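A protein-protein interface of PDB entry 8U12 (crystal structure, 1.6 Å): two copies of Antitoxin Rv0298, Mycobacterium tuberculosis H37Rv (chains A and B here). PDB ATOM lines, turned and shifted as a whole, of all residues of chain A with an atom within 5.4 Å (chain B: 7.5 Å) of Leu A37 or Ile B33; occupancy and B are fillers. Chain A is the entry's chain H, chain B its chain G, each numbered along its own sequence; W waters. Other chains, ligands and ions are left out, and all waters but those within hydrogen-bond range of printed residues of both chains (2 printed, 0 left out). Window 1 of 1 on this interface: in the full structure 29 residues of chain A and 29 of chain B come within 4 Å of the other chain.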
ATOM      1  N   ILE A   6       0.501  24.636  31.717  1.00  0.00           N
ATOM      2  CA  ILE A   6       0.751  23.784  30.566  1.00  0.00           C
ATOM      3  C   ILE A   6       1.922  24.321  29.748  1.00  0.00           C
ATOM      4  O   ILE A   6       2.280  25.502  29.808  1.00  0.00           O
ATOM      5  CB  ILE A   6      -0.489  23.667  29.657  1.00  0.00           C
ATOM      6  CG1 ILE A   6      -0.855  25.048  29.111  1.00  0.00           C
ATOM      7  CG2 ILE A   6      -1.639  23.001  30.432  1.00  0.00           C
ATOM      8  CD1 ILE A   6      -1.869  25.018  27.967  1.00  0.00           C
ATOM      9  N   VAL A   8       3.322  24.658  25.825  1.00  0.00           N
ATOM     10  CA  VAL A   8       2.897  24.652  24.429  1.00  0.00           C
ATOM     11  C   VAL A   8       3.957  25.313  23.558  1.00  0.00           C
ATOM     12  O   VAL A   8       4.793  26.093  24.023  1.00  0.00           O
ATOM     13  CB  VAL A   8       1.552  25.370  24.211  1.00  0.00           C
ATOM     14  CG1 VAL A   8       0.418  24.619  24.904  1.00  0.00           C
ATOM     15  CG2 VAL A   8       1.658  26.748  24.726  1.00  0.00           C
ATOM     16  N   MET A  32      -3.351  37.313  28.688  1.00  0.00           N
ATOM     17  CA  MET A  32      -3.706  37.599  27.273  1.00  0.00           C
ATOM     18  C   MET A  32      -3.961  36.281  26.535  1.00  0.00           C
ATOM     19  O   MET A  32      -4.860  36.253  25.677  1.00  0.00           O
ATOM     20  CB  MET A  32      -2.576  38.412  26.616  1.00  0.00           C
ATOM     21  CG  MET A  32      -2.720  38.606  25.119  1.00  0.00           C
ATOM     22  SD  MET A  32      -4.439  39.467  24.695  1.00  0.00           S
ATOM     23  CE  MET A  32      -4.097  41.115  25.590  1.00  0.00           C
ATOM     24  N   ILE A  33      -3.206  35.224  26.851  1.00  0.00           N
ATOM     25  CA  ILE A  33      -3.510  33.945  26.215  1.00  0.00           C
ATOM     26  C   ILE A  33      -4.895  33.463  26.631  1.00  0.00           C
ATOM     27  O   ILE A  33      -5.677  32.981  25.794  1.00  0.00           O
ATOM     28  CB  ILE A  33      -2.404  32.906  26.519  1.00  0.00           C
ATOM     29  CG1 ILE A  33      -1.145  33.331  25.754  1.00  0.00           C
ATOM     30  CG2 ILE A  33      -2.888  31.512  26.059  1.00  0.00           C
ATOM     31  CD1 ILE A  33       0.096  32.452  26.000  1.00  0.00           C
ATOM     32  N   GLU A  34      -5.246  33.604  27.917  1.00  0.00           N
ATOM     33  CA  GLU A  34      -6.603  33.220  28.323  1.00  0.00           C
ATOM     34  C   GLU A  34      -7.668  34.034  27.591  1.00  0.00           C
ATOM     35  O   GLU A  34      -8.692  33.480  27.173  1.00  0.00           O
ATOM     36  CB  GLU A  34      -6.782  33.356  29.835  1.00  0.00           C
ATOM     37  CG  GLU A  34      -8.178  32.884  30.268  1.00  0.00           C
ATOM     38  CD  GLU A  34      -8.367  32.958  31.751  1.00  0.00           C
ATOM     39  OE1 GLU A  34      -7.400  32.589  32.475  1.00  0.00           O
ATOM     40  OE2 GLU A  34      -9.457  33.411  32.200  1.00  0.00           O
ATOM     41  N   GLN A  35      -7.438  35.344  27.412  1.00  0.00           N
ATOM     42  CA  GLN A  35      -8.384  36.161  26.640  1.00  0.00           C
ATOM     43  C   GLN A  35      -8.582  35.555  25.260  1.00  0.00           C
ATOM     44  O   GLN A  35      -9.716  35.459  24.750  1.00  0.00           O
ATOM     45  CB  GLN A  35      -7.818  37.600  26.538  1.00  0.00           C
ATOM     46  CG  GLN A  35      -8.707  38.522  25.707  1.00  0.00           C
ATOM     47  CD  GLN A  35      -8.183  39.943  25.711  1.00  0.00           C
ATOM     48  OE1 GLN A  35      -8.014  40.550  26.788  1.00  0.00           O
ATOM     49  NE2 GLN A  35      -8.003  40.531  24.492  1.00  0.00           N
ATOM     50  N   ALA A  36      -7.473  35.219  24.604  1.00  0.00           N
ATOM     51  CA  ALA A  36      -7.547  34.682  23.234  1.00  0.00           C
ATOM     52  C   ALA A  36      -8.274  33.355  23.200  1.00  0.00           C
ATOM     53  O   ALA A  36      -9.076  33.106  22.295  1.00  0.00           O
ATOM     54  CB  ALA A  36      -6.130  34.493  22.684  1.00  0.00           C
ATOM     55  N   LEU A  37      -8.008  32.490  24.177  1.00  0.00           N
ATOM     56  CA  LEU A  37      -8.645  31.154  24.139  1.00  0.00           C
ATOM     57  C   LEU A  37     -10.131  31.233  24.432  1.00  0.00           C
ATOM     58  O   LEU A  37     -10.919  30.446  23.863  1.00  0.00           O
ATOM     59  CB  LEU A  37      -7.965  30.190  25.127  1.00  0.00           C
ATOM     60  CG  LEU A  37      -6.453  29.968  24.946  1.00  0.00           C
ATOM     61  CD1 LEU A  37      -5.932  28.953  26.003  1.00  0.00           C
ATOM     62  CD2 LEU A  37      -6.148  29.487  23.567  1.00  0.00           C
ATOM     63  N   ARG A  38     -10.537  32.108  25.352  1.00  0.00           N
ATOM     64  CA  ARG A  38     -11.971  32.278  25.614  1.00  0.00           C
ATOM     65  C   ARG A  38     -12.680  32.793  24.366  1.00  0.00           C
ATOM     66  O   ARG A  38     -13.778  32.322  24.011  1.00  0.00           O
ATOM     67  CB  ARG A  38     -12.168  33.255  26.781  1.00  0.00           C
ATOM     68  CG  ARG A  38     -13.603  33.403  27.238  1.00  0.00           C
ATOM     69  CD  ARG A  38     -13.741  34.160  28.585  1.00  0.00           C
ATOM     70  NE  ARG A  38     -12.856  33.749  29.688  1.00  0.00           N
ATOM     71  CZ  ARG A  38     -13.177  33.000  30.750  1.00  0.00           C
ATOM     72  NH1 ARG A  38     -14.342  32.385  30.852  1.00  0.00           N
ATOM     73  NH2 ARG A  38     -12.292  32.845  31.728  1.00  0.00           N
ATOM     74  N   ASN A  39     -12.084  33.788  23.712  1.00  0.00           N
ATOM     75  CA  ASN A  39     -12.730  34.333  22.519  1.00  0.00           C
ATOM     76  C   ASN A  39     -12.693  33.355  21.365  1.00  0.00           C
ATOM     77  O   ASN A  39     -13.615  33.346  20.542  1.00  0.00           O
ATOM     78  CB  ASN A  39     -12.041  35.643  22.120  1.00  0.00           C
ATOM     79  CG  ASN A  39     -12.436  36.782  23.035  1.00  0.00           C
ATOM     80  OD1 ASN A  39     -13.498  36.761  23.666  1.00  0.00           O
ATOM     81  ND2 ASN A  39     -11.601  37.830  23.079  1.00  0.00           N
ATOM     82  N   GLU A  40     -11.636  32.550  21.252  1.00  0.00           N
ATOM     83  CA  GLU A  40     -11.604  31.653  20.099  1.00  0.00           C
ATOM     84  C   GLU A  40     -12.707  30.611  20.177  1.00  0.00           C
ATOM     85  O   GLU A  40     -13.182  30.146  19.134  1.00  0.00           O
ATOM     86  CB  GLU A  40     -10.239  30.962  19.996  1.00  0.00           C
ATOM     87  CG  GLU A  40     -10.026  30.165  18.713  1.00  0.00           C
ATOM     88  CD  GLU A  40      -9.990  31.032  17.451  1.00  0.00           C
ATOM     89  OE1 GLU A  40      -9.893  32.279  17.575  1.00  0.00           O
ATOM     90  OE2 GLU A  40     -10.096  30.463  16.346  1.00  0.00           O
ATOM     91  N   HIS A  41     -13.129  30.219  21.389  1.00  0.00           N
ATOM     92  CA  HIS A  41     -14.235  29.271  21.503  1.00  0.00           C
ATOM     93  C   HIS A  41     -15.511  29.829  20.871  1.00  0.00           C
ATOM     94  O   HIS A  41     -16.359  29.068  20.357  1.00  0.00           O
ATOM     95  CB  HIS A  41     -14.441  28.943  22.992  1.00  0.00           C
ATOM     96  CG  HIS A  41     -15.595  28.049  23.275  1.00  0.00           C
ATOM     97  ND1 HIS A  41     -15.613  26.724  22.892  1.00  0.00           N
ATOM     98  CD2 HIS A  41     -16.757  28.273  23.929  1.00  0.00           C
ATOM     99  CE1 HIS A  41     -16.741  26.163  23.311  1.00  0.00           C
ATOM    100  NE2 HIS A  41     -17.461  27.085  23.926  1.00  0.00           N
ATOM    101  N   ILE B   6       6.717  27.469  25.536  1.00  0.00           N
ATOM    102  CA  ILE B   6       6.431  28.339  26.670  1.00  0.00           C
ATOM    103  C   ILE B   6       5.570  27.600  27.677  1.00  0.00           C
ATOM    104  O   ILE B   6       4.898  26.628  27.354  1.00  0.00           O
ATOM    105  CB  ILE B   6       5.707  29.630  26.257  1.00  0.00           C
ATOM    106  CG1 ILE B   6       4.426  29.276  25.529  1.00  0.00           C
ATOM    107  CG2 ILE B   6       6.638  30.501  25.394  1.00  0.00           C
ATOM    108  CD1 ILE B   6       3.524  30.468  25.236  1.00  0.00           C
ATOM    109  N   VAL B   8       2.457  28.334  30.345  1.00  0.00           N
ATOM    110  CA  VAL B   8       1.395  29.292  30.590  1.00  0.00           C
ATOM    111  C   VAL B   8       0.424  28.683  31.590  1.00  0.00           C
ATOM    112  O   VAL B   8       0.234  27.470  31.626  1.00  0.00           O
ATOM    113  CB  VAL B   8       0.695  29.693  29.288  1.00  0.00           C
ATOM    114  CG1 VAL B   8       0.166  28.498  28.566  1.00  0.00           C
ATOM    115  CG2 VAL B   8      -0.432  30.650  29.545  1.00  0.00           C
ATOM    116  N   VAL B  10      -3.522  28.674  32.597  1.00  0.00           N
ATOM    117  CA  VAL B  10      -4.810  29.003  31.993  1.00  0.00           C
ATOM    118  C   VAL B  10      -5.939  28.382  32.811  1.00  0.00           C
ATOM    119  O   VAL B  10      -5.806  27.279  33.345  1.00  0.00           O
ATOM    120  CB  VAL B  10      -4.886  28.534  30.518  1.00  0.00           C
ATOM    121  CG1 VAL B  10      -4.537  27.080  30.420  1.00  0.00           C
ATOM    122  CG2 VAL B  10      -6.257  28.772  29.898  1.00  0.00           C
ATOM    123  N   ASP B  11      -7.033  29.120  32.919  1.00  0.00           N
ATOM    124  CA  ASP B  11      -8.254  28.613  33.553  1.00  0.00           C
ATOM    125  C   ASP B  11      -8.651  27.238  32.996  1.00  0.00           C
ATOM    126  O   ASP B  11      -8.664  27.026  31.785  1.00  0.00           O
ATOM    127  CB  ASP B  11      -9.356  29.631  33.319  1.00  0.00           C
ATOM    128  CG  ASP B  11     -10.658  29.213  33.905  1.00  0.00           C
ATOM    129  OD1 ASP B  11     -11.417  28.493  33.214  1.00  0.00           O
ATOM    130  OD2 ASP B  11     -10.917  29.613  35.053  1.00  0.00           O
ATOM    131  N   VAL B  14     -11.632  27.179  30.514  1.00  0.00           N
ATOM    132  CA  VAL B  14     -11.231  27.759  29.221  1.00  0.00           C
ATOM    133  C   VAL B  14     -10.408  26.748  28.433  1.00  0.00           C
ATOM    134  O   VAL B  14     -10.581  26.578  27.218  1.00  0.00           O
ATOM    135  CB  VAL B  14     -10.444  29.065  29.465  1.00  0.00           C
ATOM    136  CG1 VAL B  14      -9.793  29.614  28.159  1.00  0.00           C
ATOM    137  CG2 VAL B  14     -11.375  30.101  30.116  1.00  0.00           C
ATOM    138  N   LEU B  15      -9.475  26.074  29.111  1.00  0.00           N
ATOM    139  CA  LEU B  15      -8.611  25.111  28.425  1.00  0.00           C
ATOM    140  C   LEU B  15      -9.407  23.914  27.926  1.00  0.00           C
ATOM    141  O   LEU B  15      -9.201  23.427  26.805  1.00  0.00           O
ATOM    142  CB  LEU B  15      -7.513  24.624  29.383  1.00  0.00           C
ATOM    143  CG  LEU B  15      -6.504  23.687  28.735  1.00  0.00           C
ATOM    144  CD1 LEU B  15      -5.832  24.396  27.558  1.00  0.00           C
ATOM    145  CD2 LEU B  15      -5.447  23.266  29.762  1.00  0.00           C
ATOM    146  N   ALA B  17     -12.488  23.790  27.079  1.00  0.00           N
ATOM    147  CA  ALA B  17     -13.336  24.161  25.952  1.00  0.00           C
ATOM    148  C   ALA B  17     -12.523  24.268  24.677  1.00  0.00           C
ATOM    149  O   ALA B  17     -12.958  23.815  23.614  1.00  0.00           O
ATOM    150  CB  ALA B  17     -14.057  25.487  26.269  1.00  0.00           C
ATOM    151  N   ILE B  18     -11.347  24.887  24.739  1.00  0.00           N
ATOM    152  CA  ILE B  18     -10.612  25.035  23.484  1.00  0.00           C
ATOM    153  C   ILE B  18      -9.959  23.697  23.093  1.00  0.00           C
ATOM    154  O   ILE B  18      -9.775  23.410  21.897  1.00  0.00           O
ATOM    155  CB  ILE B  18      -9.633  26.227  23.594  1.00  0.00           C
ATOM    156  CG1 ILE B  18      -9.231  26.797  22.210  1.00  0.00           C
ATOM    157  CG2 ILE B  18      -8.417  25.832  24.369  1.00  0.00           C
ATOM    158  CD1 ILE B  18     -10.370  27.564  21.489  1.00  0.00           C
ATOM    159  N   ASP B  19      -9.660  22.818  24.062  1.00  0.00           N
ATOM    160  CA  ASP B  19      -9.230  21.468  23.696  1.00  0.00           C
ATOM    161  C   ASP B  19     -10.345  20.723  22.964  1.00  0.00           C
ATOM    162  O   ASP B  19     -10.086  19.980  22.001  1.00  0.00           O
ATOM    163  CB  ASP B  19      -8.860  20.648  24.928  1.00  0.00           C
ATOM    164  CG  ASP B  19      -7.444  20.936  25.477  1.00  0.00           C
ATOM    165  OD1 ASP B  19      -6.574  21.467  24.744  1.00  0.00           O
ATOM    166  OD2 ASP B  19      -7.193  20.563  26.659  1.00  0.00           O
ATOM    167  N   ASP B  21     -12.623  22.122  21.145  1.00  0.00           N
ATOM    168  CA  ASP B  21     -12.678  22.691  19.794  1.00  0.00           C
ATOM    169  C   ASP B  21     -11.539  22.162  18.939  1.00  0.00           C
ATOM    170  O   ASP B  21     -11.704  21.959  17.731  1.00  0.00           O
ATOM    171  CB  ASP B  21     -12.622  24.224  19.841  1.00  0.00           C
ATOM    172  CG  ASP B  21     -13.870  24.852  20.474  1.00  0.00           C
ATOM    173  OD1 ASP B  21     -15.016  24.367  20.238  1.00  0.00           O
ATOM    174  OD2 ASP B  21     -13.715  25.887  21.163  1.00  0.00           O
ATOM    175  N   ALA B  22     -10.351  22.009  19.529  1.00  0.00           N
ATOM    176  CA  ALA B  22      -9.227  21.468  18.775  1.00  0.00           C
ATOM    177  C   ALA B  22      -9.542  20.081  18.264  1.00  0.00           C
ATOM    178  O   ALA B  22      -9.310  19.768  17.095  1.00  0.00           O
ATOM    179  CB  ALA B  22      -7.967  21.427  19.671  1.00  0.00           C
ATOM    180  N   LEU B  27      -7.101  19.500  15.176  1.00  0.00           N
ATOM    181  CA  LEU B  27      -5.856  20.185  15.512  1.00  0.00           C
ATOM    182  C   LEU B  27      -5.322  19.652  16.831  1.00  0.00           C
ATOM    183  O   LEU B  27      -6.109  19.238  17.695  1.00  0.00           O
ATOM    184  CB  LEU B  27      -6.089  21.695  15.638  1.00  0.00           C
ATOM    185  CG  LEU B  27      -6.511  22.416  14.351  1.00  0.00           C
ATOM    186  CD1 LEU B  27      -6.633  23.933  14.590  1.00  0.00           C
ATOM    187  CD2 LEU B  27      -5.498  22.155  13.266  1.00  0.00           C
ATOM    188  N   ASN B  28      -3.997  19.678  17.013  1.00  0.00           N
ATOM    189  CA  ASN B  28      -3.515  19.444  18.364  1.00  0.00           C
ATOM    190  C   ASN B  28      -3.617  20.731  19.200  1.00  0.00           C
ATOM    191  O   ASN B  28      -4.002  21.800  18.718  1.00  0.00           O
ATOM    192  CB  ASN B  28      -2.103  18.854  18.360  1.00  0.00           C
ATOM    193  CG  ASN B  28      -1.069  19.782  17.798  1.00  0.00           C
ATOM    194  OD1 ASN B  28      -1.090  20.993  18.050  1.00  0.00           O
ATOM    195  ND2 ASN B  28      -0.101  19.214  17.059  1.00  0.00           N
ATOM    196  N   ARG B  29      -3.281  20.628  20.484  1.00  0.00           N
ATOM    197  CA  ARG B  29      -3.475  21.775  21.367  1.00  0.00           C
ATOM    198  C   ARG B  29      -2.651  22.979  20.921  1.00  0.00           C
ATOM    199  O   ARG B  29      -3.159  24.118  20.915  1.00  0.00           O
ATOM    200  CB  ARG B  29      -3.090  21.410  22.789  1.00  0.00           C
ATOM    201  CG  ARG B  29      -3.318  22.584  23.741  1.00  0.00           C
ATOM    202  CD  ARG B  29      -2.881  22.198  25.131  1.00  0.00           C
ATOM    203  NE  ARG B  29      -3.855  21.364  25.828  1.00  0.00           N
ATOM    204  CZ  ARG B  29      -3.626  20.779  26.994  1.00  0.00           C
ATOM    205  NH1 ARG B  29      -2.418  20.763  27.528  1.00  0.00           N
ATOM    206  NH2 ARG B  29      -4.621  20.160  27.620  1.00  0.00           N
ATOM    207  N   SER B  30      -1.362  22.765  20.622  1.00  0.00           N
ATOM    208  CA  SER B  30      -0.524  23.907  20.246  1.00  0.00           C
ATOM    209  C   SER B  30      -1.027  24.562  18.962  1.00  0.00           C
ATOM    210  O   SER B  30      -1.011  25.797  18.847  1.00  0.00           O
ATOM    211  CB  SER B  30       0.940  23.475  20.103  1.00  0.00           C
ATOM    212  OG  SER B  30       1.489  23.230  21.404  1.00  0.00           O
ATOM    213  N   GLU B  31      -1.491  23.756  17.992  1.00  0.00           N
ATOM    214  CA  GLU B  31      -2.014  24.336  16.757  1.00  0.00           C
ATOM    215  C   GLU B  31      -3.246  25.186  17.019  1.00  0.00           C
ATOM    216  O   GLU B  31      -3.440  26.242  16.392  1.00  0.00           O
ATOM    217  CB  GLU B  31      -2.377  23.240  15.755  1.00  0.00           C
ATOM    218  CG  GLU B  31      -1.147  22.515  15.195  1.00  0.00           C
ATOM    219  CD  GLU B  31      -1.447  21.211  14.475  1.00  0.00           C
ATOM    220  OE1 GLU B  31      -2.500  20.547  14.700  1.00  0.00           O
ATOM    221  OE2 GLU B  31      -0.573  20.799  13.677  1.00  0.00           O
ATOM    222  N   MET B  32      -4.134  24.704  17.868  1.00  0.00           N
ATOM    223  CA  MET B  32      -5.356  25.497  18.159  1.00  0.00           C
ATOM    224  C   MET B  32      -4.987  26.723  18.992  1.00  0.00           C
ATOM    225  O   MET B  32      -5.613  27.781  18.800  1.00  0.00           O
ATOM    226  CB  MET B  32      -6.406  24.650  18.887  1.00  0.00           C
ATOM    227  CG  MET B  32      -7.636  25.490  19.291  1.00  0.00           C
ATOM    228  SD  MET B  32      -8.551  26.452  17.822  1.00  0.00           S
ATOM    229  CE  MET B  32      -9.562  24.911  17.162  1.00  0.00           C
ATOM    230  N   ILE B  33      -4.018  26.634  19.893  1.00  0.00           N
ATOM    231  CA  ILE B  33      -3.675  27.840  20.634  1.00  0.00           C
ATOM    232  C   ILE B  33      -3.079  28.879  19.688  1.00  0.00           C
ATOM    233  O   ILE B  33      -3.381  30.078  19.791  1.00  0.00           O
ATOM    234  CB  ILE B  33      -2.718  27.495  21.790  1.00  0.00           C
ATOM    235  CG1 ILE B  33      -3.523  26.749  22.844  1.00  0.00           C
ATOM    236  CG2 ILE B  33      -2.052  28.793  22.365  1.00  0.00           C
ATOM    237  CD1 ILE B  33      -2.715  26.202  24.033  1.00  0.00           C
ATOM    238  N   GLU B  34      -2.221  28.439  18.758  1.00  0.00           N
ATOM    239  CA  GLU B  34      -1.668  29.373  17.783  1.00  0.00           C
ATOM    240  C   GLU B  34      -2.777  30.042  16.984  1.00  0.00           C
ATOM    241  O   GLU B  34      -2.735  31.254  16.732  1.00  0.00           O
ATOM    242  CB  GLU B  34      -0.674  28.642  16.866  1.00  0.00           C
ATOM    243  CG  GLU B  34       0.113  29.586  16.024  1.00  0.00           C
ATOM    244  CD  GLU B  34       1.251  28.883  15.331  1.00  0.00           C
ATOM    245  OE1 GLU B  34       2.091  28.238  16.027  1.00  0.00           O
ATOM    246  OE2 GLU B  34       1.273  28.975  14.084  1.00  0.00           O
ATOM    247  N   GLN B  35      -3.793  29.270  16.569  1.00  0.00           N
ATOM    248  CA  GLN B  35      -4.888  29.867  15.827  1.00  0.00           C
ATOM    249  C   GLN B  35      -5.586  30.940  16.673  1.00  0.00           C
ATOM    250  O   GLN B  35      -5.946  32.015  16.160  1.00  0.00           O
ATOM    251  CB  GLN B  35      -5.872  28.774  15.417  1.00  0.00           C
ATOM    252  CG  GLN B  35      -7.167  29.308  14.768  1.00  0.00           C
ATOM    253  CD  GLN B  35      -8.072  28.157  14.376  1.00  0.00           C
ATOM    254  OE1 GLN B  35      -7.639  27.236  13.659  1.00  0.00           O
ATOM    255  NE2 GLN B  35      -9.351  28.185  14.827  1.00  0.00           N
ATOM    256  N   ALA B  36      -5.866  30.612  17.939  1.00  0.00           N
ATOM    257  CA  ALA B  36      -6.513  31.565  18.834  1.00  0.00           C
ATOM    258  C   ALA B  36      -5.696  32.846  18.968  1.00  0.00           C
ATOM    259  O   ALA B  36      -6.262  33.957  18.987  1.00  0.00           O
ATOM    260  CB  ALA B  36      -6.712  30.944  20.229  1.00  0.00           C
ATOM    261  N   LEU B  37      -4.374  32.707  19.078  1.00  0.00           N
ATOM    262  CA  LEU B  37      -3.534  33.890  19.291  1.00  0.00           C
ATOM    263  C   LEU B  37      -3.503  34.748  18.045  1.00  0.00           C
ATOM    264  O   LEU B  37      -3.517  35.983  18.142  1.00  0.00           O
ATOM    265  CB  LEU B  37      -2.095  33.469  19.659  1.00  0.00           C
ATOM    266  CG  LEU B  37      -2.010  32.740  20.991  1.00  0.00           C
ATOM    267  CD1 LEU B  37      -0.531  32.474  21.283  1.00  0.00           C
ATOM    268  CD2 LEU B  37      -2.604  33.559  22.109  1.00  0.00           C
ATOM    269  N   ARG B  38      -3.375  34.128  16.867  1.00  0.00           N
ATOM    270  CA  ARG B  38      -3.412  34.889  15.614  1.00  0.00           C
ATOM    271  C   ARG B  38      -4.717  35.664  15.496  1.00  0.00           C
ATOM    272  O   ARG B  38      -4.722  36.858  15.157  1.00  0.00           O
ATOM    273  CB  ARG B  38      -3.274  33.961  14.405  1.00  0.00           C
ATOM    274  CG  ARG B  38      -1.874  33.469  14.077  1.00  0.00           C
ATOM    275  CD  ARG B  38      -1.915  32.726  12.701  1.00  0.00           C
ATOM    276  NE  ARG B  38      -1.789  33.542  11.483  1.00  0.00           N
ATOM    277  CZ  ARG B  38      -2.740  33.732  10.563  1.00  0.00           C
ATOM    278  NH1 ARG B  38      -3.980  33.307  10.739  1.00  0.00           N
ATOM    279  NH2 ARG B  38      -2.434  34.358   9.428  1.00  0.00           N
ATOM    280  N   ASN B  39      -5.851  34.985  15.730  1.00  0.00           N
ATOM    281  CA  ASN B  39      -7.119  35.675  15.596  1.00  0.00           C
ATOM    282  C   ASN B  39      -7.311  36.757  16.656  1.00  0.00           C
ATOM    283  O   ASN B  39      -8.029  37.745  16.402  1.00  0.00           O
ATOM    284  CB  ASN B  39      -8.252  34.652  15.652  1.00  0.00           C
ATOM    285  CG  ASN B  39      -8.209  33.704  14.451  1.00  0.00           C
ATOM    286  OD1 ASN B  39      -7.624  34.057  13.411  1.00  0.00           O
ATOM    287  ND2 ASN B  39      -8.861  32.541  14.543  1.00  0.00           N
ATOM    288  N   GLU B  40      -6.792  36.539  17.866  1.00  0.00           N
ATOM    289  CA  GLU B  40      -6.923  37.573  18.880  1.00  0.00           C
ATOM    290  C   GLU B  40      -6.070  38.781  18.511  1.00  0.00           C
ATOM    291  O   GLU B  40      -6.470  39.914  18.771  1.00  0.00           O
ATOM    292  CB  GLU B  40      -6.524  37.021  20.250  1.00  0.00           C
ATOM    293  CG  GLU B  40      -6.908  37.961  21.403  1.00  0.00           C
ATOM    294  CD  GLU B  40      -8.416  38.146  21.554  1.00  0.00           C
ATOM    295  OE1 GLU B  40      -9.225  37.299  21.063  1.00  0.00           O
ATOM    296  OE2 GLU B  40      -8.827  39.135  22.201  1.00  0.00           O
HETATM  297  O   HOH W   1     -12.093  28.483  25.599  1.00  0.00           O
HETATM  298  O   HOH W   2     -17.092  26.318  19.911  1.00  0.00           O
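Ile A6 touches Val B8, and with the chains exchanged Val A8 touches Ile B6. Gln A35 touches Glu B40, and with the chains exchanged Glu A40 touches Gln B35. Ala B36 touches its own counterpart, Ala A36. Asn A39 touches Glu B40, and with the chains exchanged Glu A40 touches Asn B39. Positions printed for both chains: 6, 8, 32, 33, 34, 35, 36, 37, 38, 39 and 40. Of the 27 pairs that touch across the chains among the printed residues, 14 have their exchanged pair printed and touching as well.
Water W2 lies within hydrogen-bond range of the side-chain carboxylate of Asp B21 (2.9 Å) and the backbone carbonyl oxygen of His A41 (2.9 Å). Water W1 bridges the backbone carbonyl oxygen (O) of Leu A37 (2.9 Å) and the backbone carbonyl oxygen (O) of Val B14 (2.9 Å).
Hydrophobic or aromatic side chains of chain A within 4 Å of the printed part of chain B: Ile A6, Val A8, Ile A33, Ala A36, Leu A37 and His A41. Of the 25 printed residues of chain B, 17 touch a printed residue of chain A. Hydrophobic or aromatic side chains of chain B within 4 Å of the printed part of chain A: Ile B6, Val B8, Val B10, Val B14, Leu B15, Ala B17, Ile B18, Ile B33, Ala B36 and Leu B37. Among the printed residues, 27 pairs touch across the chains.
The side-chain amide oxygen (OD1) of Asn B28 sits at hydrogen-bond distance from the backbone NH (N) of Ser B30 (3.1 Å). The backbone carbonyl oxygen (O) of Gln B35 sits close to the side-chain amide nitrogen (ND2) of Asn B39 (3.4 Å). The side-chain sulfur (SD) of Met B32 is in hydrogen-bond range of the side-chain amide nitrogen (NE2) of Gln B35 (3.6 Å). ND2 of Asn A39 sits at hydrogen-bond distance from O of Gln A35, 3.5 Å away. The backbone NH (N) of Val B14 lies within hydrogen-bond range of the side-chain carboxylate (OD1) of Asp B11 (3.0 Å). NH2 of Arg B29 is in salt-bridge range of OD2 of Asp B19.
The side-chain carboxylate of Glu A40 lies within hydrogen-bond range of the side-chain amide nitrogen of Gln B35 (2.8 Å). The backbone NH of Ile A6 lies within hydrogen-bond range of the backbone carbonyl oxygen of Val B8 (2.8 Å). The backbone NH (N) of Ile B6 sits at hydrogen-bond distance from the backbone carbonyl oxygen (O) of Val A8. OE1 of Glu B40 lies within hydrogen-bond range of ND2 of Asn A39. ND2 of Asn B39 is in hydrogen-bond range of OE2 of Glu A40, at 3.0 Å. OD2 of Asp B21 lies within hydrogen-bond range of ND1 of His A41 (2.7 Å). The side-chain amide nitrogen (NE2) of Gln A35 lies within hydrogen-bond range of the side-chain carboxylate (OE2) of Glu B40, 2.8 Å away.
CD2 of Leu B15 touches CG2 of Ile A6, at 3.9 Å. Arg B29 touches Ile A6. CD2 of Leu B37 touches CG1 of Ile A33, 3.9 Å away. Ala A36 touches Ala B36 (CB to O, 3.7 Å). Leu A37 touches Val B10. Leu A37 touches Ile B18. CG1 of Ile B33 touches CD2 of Leu A37, at 3.9 Å. Leu A37 touches Ala B36. NH2 of Arg A38 touches CG2 of Val B14, 3.3 Å away. His A41 touches Ile B18.
Ala A36 touches just these residues of chain B: Ala B36, Leu B37 and Glu B40. Printed residues of chain B within 4 Å of Asn A39: Glu B40 (3.2 Å). Printed residues of chain A within 4 Å of Leu B15: Ile A6 (3.9 Å). Ile B33 touches two residues of chain A. Glu B34 touches none of the printed residues of chain A. Printed residues of chain A within 4 Å of Glu B40: Gln A35, Ala A36 and Asn A39. The nearest residue of chain B that does not touch Leu A37 is Leu B15 (4.8 Å). The nearest residue of chain A that does not touch Ile B33 is Ile A6 (4.2 Å). The nearest printed residue of chain B that does not touch Gln A35 is Val B14 (6.2 Å).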
